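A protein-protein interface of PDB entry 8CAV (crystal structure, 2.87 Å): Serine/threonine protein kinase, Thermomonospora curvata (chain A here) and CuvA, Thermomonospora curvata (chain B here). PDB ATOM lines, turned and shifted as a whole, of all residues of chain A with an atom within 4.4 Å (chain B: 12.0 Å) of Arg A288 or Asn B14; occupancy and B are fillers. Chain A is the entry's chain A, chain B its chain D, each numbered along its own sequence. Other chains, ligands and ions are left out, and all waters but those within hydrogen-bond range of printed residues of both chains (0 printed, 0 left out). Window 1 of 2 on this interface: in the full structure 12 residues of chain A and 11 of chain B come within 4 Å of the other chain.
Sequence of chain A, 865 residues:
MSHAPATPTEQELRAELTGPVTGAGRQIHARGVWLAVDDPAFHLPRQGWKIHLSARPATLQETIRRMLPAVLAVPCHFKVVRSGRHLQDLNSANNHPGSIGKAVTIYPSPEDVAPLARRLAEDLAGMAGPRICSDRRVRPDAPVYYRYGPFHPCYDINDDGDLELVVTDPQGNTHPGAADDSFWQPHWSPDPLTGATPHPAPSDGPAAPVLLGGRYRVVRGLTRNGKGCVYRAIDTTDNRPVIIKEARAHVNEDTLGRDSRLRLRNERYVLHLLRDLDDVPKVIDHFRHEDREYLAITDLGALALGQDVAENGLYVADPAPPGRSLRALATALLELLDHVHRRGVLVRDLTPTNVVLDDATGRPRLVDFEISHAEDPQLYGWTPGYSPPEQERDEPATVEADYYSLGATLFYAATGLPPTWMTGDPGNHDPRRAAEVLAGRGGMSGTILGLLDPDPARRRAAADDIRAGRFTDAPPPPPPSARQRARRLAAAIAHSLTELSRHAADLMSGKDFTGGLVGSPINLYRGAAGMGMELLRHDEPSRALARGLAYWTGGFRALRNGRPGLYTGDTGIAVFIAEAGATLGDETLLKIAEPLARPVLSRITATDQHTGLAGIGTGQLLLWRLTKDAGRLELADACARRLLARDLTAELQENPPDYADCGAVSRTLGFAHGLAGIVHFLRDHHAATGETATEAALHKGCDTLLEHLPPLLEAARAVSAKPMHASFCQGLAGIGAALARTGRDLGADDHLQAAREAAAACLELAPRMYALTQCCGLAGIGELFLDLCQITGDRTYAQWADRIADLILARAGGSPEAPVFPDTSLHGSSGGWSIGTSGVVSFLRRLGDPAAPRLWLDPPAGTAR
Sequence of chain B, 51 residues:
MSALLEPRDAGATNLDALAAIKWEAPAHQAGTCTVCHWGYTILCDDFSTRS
Of chain B, only Asn B14 and Leu B15 come within 4 Å of His A286. Printed residues of chain B within 4 Å of His A289: Leu B18 and Ala B20. Asn B14 touches just these residues of chain A: His A286, Phe A287, Arg A288 and Glu A293. Of the printed residues of chain A, Asp B16 touches Arg A288. Printed residues of chain A within 4 Å of Ala B17: Arg A288. Printed residues of chain A within 4 Å of Leu B18: Arg A288 (3.5 Å) and His A289 (3.1 Å). Of the printed residues of chain A, Ala B20 touches His A289 (3.7 Å) and Glu A290 (3.1 Å). The nearest printed residue of chain A that does not touch Ala B17 is Glu A290 (4.4 Å).
NE2 of His A286 lies close to OE2 of Glu A293 (3.1 Å).
Of the 7 printed residues of chain A, 6 touch a printed residue of chain B. Hydrophobic or aromatic side chains of chain A that line the printed part of chain B: His A286 and His A289. Of the 13 printed residues of chain B, 6 touch a printed residue of chain A. Printed residues of chain B that touch a printed residue of chain A: Asn B14, Leu B15, Asp B16, Ala B17, Leu B18 and Ala B20. Hydrophobic or aromatic side chains of chain B that line the printed part of chain A: Leu B15, Ala B17, Leu B18 and Ala B20. Among the printed residues, no Asp or Glu carboxylate lies within 4 Å of a Lys or Arg side-chain nitrogen of the other chain.
His A286 touches Leu B15. O of Asn B14 touches N of Arg A288, 3.5 Å away. CG of Arg A288 touches O of Leu B15 (3.2 Å). Arg A288 touches Ala B17. Arg A288 touches Leu B18. Ala B20 touches His A289. Glu A290 touches Ala B20. CB of Asn B14 touches OE1 of Glu A293 (3.7 Å).
The backbone carbonyl oxygen (O) of His A286 sits close to the backbone carbonyl oxygen (O) of Asn B14 (2.7 Å). N of Phe A287 sits close to O of Asn B14 (3.2 Å). ND1 of His A289 is in hydrogen-bond range of O of Leu B18, at 3.1 Å. O of Arg A288 lies close to O of Asp B16 (3.4 Å).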
ATOM      1  N   HIS A 286      29.062   2.334  14.758  1.00  0.00           N
ATOM      2  CA  HIS A 286      29.286   1.157  13.921  1.00  0.00           C
ATOM      3  C   HIS A 286      28.018   0.312  13.955  1.00  0.00           C
ATOM      4  O   HIS A 286      27.544  -0.042  15.039  1.00  0.00           O
ATOM      5  CB  HIS A 286      30.487   0.338  14.409  1.00  0.00           C
ATOM      6  CG  HIS A 286      30.854  -0.814  13.517  1.00  0.00           C
ATOM      7  ND1 HIS A 286      32.147  -1.293  13.432  1.00  0.00           N
ATOM      8  CD2 HIS A 286      30.109  -1.585  12.688  1.00  0.00           C
ATOM      9  CE1 HIS A 286      32.181  -2.305  12.585  1.00  0.00           C
ATOM     10  NE2 HIS A 286      30.959  -2.505  12.125  1.00  0.00           N
ATOM     11  N   PHE A 287      27.471  -0.007  12.778  1.00  0.00           N
ATOM     12  CA  PHE A 287      26.241  -0.786  12.674  1.00  0.00           C
ATOM     13  C   PHE A 287      26.310  -1.713  11.470  1.00  0.00           C
ATOM     14  O   PHE A 287      26.891  -1.369  10.442  1.00  0.00           O
ATOM     15  CB  PHE A 287      25.007   0.125  12.531  1.00  0.00           C
ATOM     16  CG  PHE A 287      25.236   1.321  11.648  1.00  0.00           C
ATOM     17  CD1 PHE A 287      25.895   2.433  12.140  1.00  0.00           C
ATOM     18  CD2 PHE A 287      24.797   1.335  10.334  1.00  0.00           C
ATOM     19  CE1 PHE A 287      26.118   3.534  11.340  1.00  0.00           C
ATOM     20  CE2 PHE A 287      25.015   2.440   9.529  1.00  0.00           C
ATOM     21  CZ  PHE A 287      25.675   3.539  10.034  1.00  0.00           C
ATOM     22  N   ARG A 288      25.698  -2.895  11.594  1.00  0.00           N
ATOM     23  CA  ARG A 288      25.471  -3.757  10.441  1.00  0.00           C
ATOM     24  C   ARG A 288      23.994  -3.746  10.064  1.00  0.00           C
ATOM     25  O   ARG A 288      23.116  -3.634  10.926  1.00  0.00           O
ATOM     26  CB  ARG A 288      25.913  -5.208  10.694  1.00  0.00           C
ATOM     27  CG  ARG A 288      25.205  -5.932  11.836  1.00  0.00           C
ATOM     28  CD  ARG A 288      25.635  -7.400  11.921  1.00  0.00           C
ATOM     29  NE  ARG A 288      24.588  -8.317  11.480  1.00  0.00           N
ATOM     30  CZ  ARG A 288      23.852  -9.072  12.288  1.00  0.00           C
ATOM     31  NH1 ARG A 288      24.023  -9.057  13.601  1.00  0.00           N
ATOM     32  NH2 ARG A 288      22.922  -9.865  11.764  1.00  0.00           N
ATOM     33  N   HIS A 289      23.740  -3.847   8.760  1.00  0.00           N
ATOM     34  CA  HIS A 289      22.412  -4.074   8.202  1.00  0.00           C
ATOM     35  C   HIS A 289      22.443  -5.381   7.428  1.00  0.00           C
ATOM     36  O   HIS A 289      23.160  -5.482   6.428  1.00  0.00           O
ATOM     37  CB  HIS A 289      21.993  -2.964   7.238  1.00  0.00           C
ATOM     38  CG  HIS A 289      21.607  -1.686   7.899  1.00  0.00           C
ATOM     39  ND1 HIS A 289      20.748  -1.628   8.973  1.00  0.00           N
ATOM     40  CD2 HIS A 289      21.938  -0.406   7.611  1.00  0.00           C
ATOM     41  CE1 HIS A 289      20.582  -0.369   9.333  1.00  0.00           C
ATOM     42  NE2 HIS A 289      21.291   0.393   8.521  1.00  0.00           N
ATOM     43  N   GLU A 290      21.645  -6.358   7.849  1.00  0.00           N
ATOM     44  CA  GLU A 290      21.602  -7.632   7.135  1.00  0.00           C
ATOM     45  C   GLU A 290      23.017  -8.148   6.880  1.00  0.00           C
ATOM     46  O   GLU A 290      23.606  -8.774   7.768  1.00  0.00           O
ATOM     47  CB  GLU A 290      20.803  -7.474   5.837  1.00  0.00           C
ATOM     48  CG  GLU A 290      19.285  -7.433   6.065  1.00  0.00           C
ATOM     49  CD  GLU A 290      18.537  -6.648   5.003  1.00  0.00           C
ATOM     50  OE1 GLU A 290      18.537  -5.400   5.074  1.00  0.00           O
ATOM     51  OE2 GLU A 290      17.948  -7.279   4.101  1.00  0.00           O
ATOM     52  N   ARG A 292      25.695  -6.139   5.358  1.00  0.00           N
ATOM     53  CA  ARG A 292      26.583  -5.032   5.045  1.00  0.00           C
ATOM     54  C   ARG A 292      26.975  -4.344   6.340  1.00  0.00           C
ATOM     55  O   ARG A 292      26.108  -3.986   7.141  1.00  0.00           O
ATOM     56  CB  ARG A 292      25.912  -4.029   4.113  1.00  0.00           C
ATOM     57  CG  ARG A 292      25.289  -4.649   2.890  1.00  0.00           C
ATOM     58  CD  ARG A 292      24.555  -3.589   2.103  1.00  0.00           C
ATOM     59  NE  ARG A 292      25.138  -3.378   0.785  1.00  0.00           N
ATOM     60  CZ  ARG A 292      24.561  -3.742  -0.353  1.00  0.00           C
ATOM     61  NH1 ARG A 292      23.371  -4.318  -0.371  1.00  0.00           N
ATOM     62  NH2 ARG A 292      25.192  -3.515  -1.501  1.00  0.00           N
ATOM     63  N   GLU A 293      28.268  -4.150   6.538  1.00  0.00           N
ATOM     64  CA  GLU A 293      28.774  -3.492   7.729  1.00  0.00           C
ATOM     65  C   GLU A 293      29.057  -2.030   7.416  1.00  0.00           C
ATOM     66  O   GLU A 293      29.391  -1.678   6.283  1.00  0.00           O
ATOM     67  CB  GLU A 293      30.033  -4.191   8.227  1.00  0.00           C
ATOM     68  CG  GLU A 293      30.198  -4.122   9.721  1.00  0.00           C
ATOM     69  CD  GLU A 293      31.082  -5.225  10.253  1.00  0.00           C
ATOM     70  OE1 GLU A 293      30.629  -6.388  10.282  1.00  0.00           O
ATOM     71  OE2 GLU A 293      32.236  -4.933  10.632  1.00  0.00           O
ATOM     72  N   ALA B  10      37.459  -9.494  21.084  1.00  0.00           N
ATOM     73  CA  ALA B  10      36.477  -9.187  20.005  1.00  0.00           C
ATOM     74  C   ALA B  10      35.337  -8.342  20.564  1.00  0.00           C
ATOM     75  O   ALA B  10      34.162  -8.684  20.415  1.00  0.00           O
ATOM     76  CB  ALA B  10      35.946 -10.468  19.382  1.00  0.00           C
ATOM     77  N   GLY B  11      35.705  -7.246  21.223  1.00  0.00           N
ATOM     78  CA  GLY B  11      34.748  -6.252  21.691  1.00  0.00           C
ATOM     79  C   GLY B  11      34.382  -5.247  20.607  1.00  0.00           C
ATOM     80  O   GLY B  11      33.549  -4.365  20.858  1.00  0.00           O
ATOM     81  N   ALA B  12      34.980  -5.357  19.421  1.00  0.00           N
ATOM     82  CA  ALA B  12      34.637  -4.521  18.274  1.00  0.00           C
ATOM     83  C   ALA B  12      33.691  -5.316  17.376  1.00  0.00           C
ATOM     84  O   ALA B  12      34.100  -5.951  16.403  1.00  0.00           O
ATOM     85  CB  ALA B  12      35.899  -4.086  17.529  1.00  0.00           C
ATOM     86  N   THR B  13      32.409  -5.287  17.723  1.00  0.00           N
ATOM     87  CA  THR B  13      31.372  -5.985  16.981  1.00  0.00           C
ATOM     88  C   THR B  13      30.459  -4.981  16.287  1.00  0.00           C
ATOM     89  O   THR B  13      30.406  -3.804  16.652  1.00  0.00           O
ATOM     90  CB  THR B  13      30.549  -6.896  17.905  1.00  0.00           C
ATOM     91  N   ASN B  14      29.719  -5.474  15.289  1.00  0.00           N
ATOM     92  CA  ASN B  14      29.047  -4.585  14.345  1.00  0.00           C
ATOM     93  C   ASN B  14      27.894  -3.801  14.971  1.00  0.00           C
ATOM     94  O   ASN B  14      27.638  -2.670  14.552  1.00  0.00           O
ATOM     95  CB  ASN B  14      28.535  -5.406  13.157  1.00  0.00           C
ATOM     96  N   LEU B  15      27.200  -4.389  15.949  1.00  0.00           N
ATOM     97  CA  LEU B  15      26.019  -3.833  16.610  1.00  0.00           C
ATOM     98  C   LEU B  15      24.737  -4.179  15.859  1.00  0.00           C
ATOM     99  O   LEU B  15      24.769  -4.530  14.674  1.00  0.00           O
ATOM    100  CB  LEU B  15      26.111  -2.308  16.771  1.00  0.00           C
ATOM    101  N   ASP B  16      23.604  -4.033  16.546  1.00  0.00           N
ATOM    102  CA  ASP B  16      22.364  -4.684  16.154  1.00  0.00           C
ATOM    103  C   ASP B  16      22.035  -4.487  14.682  1.00  0.00           C
ATOM    104  O   ASP B  16      22.153  -3.385  14.141  1.00  0.00           O
ATOM    105  CB  ASP B  16      21.212  -4.145  17.012  1.00  0.00           C
ATOM    106  N   ALA B  17      21.607  -5.576  14.044  1.00  0.00           N
ATOM    107  CA  ALA B  17      21.066  -5.501  12.698  1.00  0.00           C
ATOM    108  C   ALA B  17      19.799  -4.658  12.688  1.00  0.00           C
ATOM    109  O   ALA B  17      18.968  -4.750  13.593  1.00  0.00           O
ATOM    110  CB  ALA B  17      20.756  -6.907  12.174  1.00  0.00           C
ATOM    111  N   LEU B  18      19.653  -3.836  11.650  1.00  0.00           N
ATOM    112  CA  LEU B  18      18.478  -3.000  11.467  1.00  0.00           C
ATOM    113  C   LEU B  18      17.901  -3.243  10.079  1.00  0.00           C
ATOM    114  O   LEU B  18      18.566  -3.780   9.194  1.00  0.00           O
ATOM    115  CB  LEU B  18      18.823  -1.518  11.656  1.00  0.00           C
ATOM    116  N   ALA B  19      16.639  -2.847   9.902  1.00  0.00           N
ATOM    117  CA  ALA B  19      15.983  -2.971   8.609  1.00  0.00           C
ATOM    118  C   ALA B  19      16.587  -1.962   7.637  1.00  0.00           C
ATOM    119  O   ALA B  19      16.610  -0.761   7.922  1.00  0.00           O
ATOM    120  CB  ALA B  19      14.480  -2.747   8.753  1.00  0.00           C
ATOM    121  N   ALA B  20      17.077  -2.442   6.501  1.00  0.00           N
ATOM    122  CA  ALA B  20      17.798  -1.600   5.559  1.00  0.00           C
ATOM    123  C   ALA B  20      16.918  -1.227   4.378  1.00  0.00           C
ATOM    124  O   ALA B  20      16.217  -2.072   3.816  1.00  0.00           O
ATOM    125  CB  ALA B  20      19.059  -2.302   5.046  1.00  0.00           C
ATOM    126  N   ILE B  21      16.982   0.046   3.994  1.00  0.00           N
ATOM    127  CA  ILE B  21      16.256   0.581   2.857  1.00  0.00           C
ATOM    128  C   ILE B  21      17.112   0.654   1.602  1.00  0.00           C
ATOM    129  O   ILE B  21      16.665   1.208   0.589  1.00  0.00           O
ATOM    130  CB  ILE B  21      15.716   1.973   3.201  1.00  0.00           C
ATOM    131  N   LYS B  22      18.329   0.111   1.643  1.00  0.00           N
ATOM    132  CA  LYS B  22      19.271   0.270   0.544  1.00  0.00           C
ATOM    133  C   LYS B  22      18.657  -0.213  -0.761  1.00  0.00           C
ATOM    134  O   LYS B  22      18.127  -1.323  -0.838  1.00  0.00           O
ATOM    135  CB  LYS B  22      20.559  -0.504   0.838  1.00  0.00           C
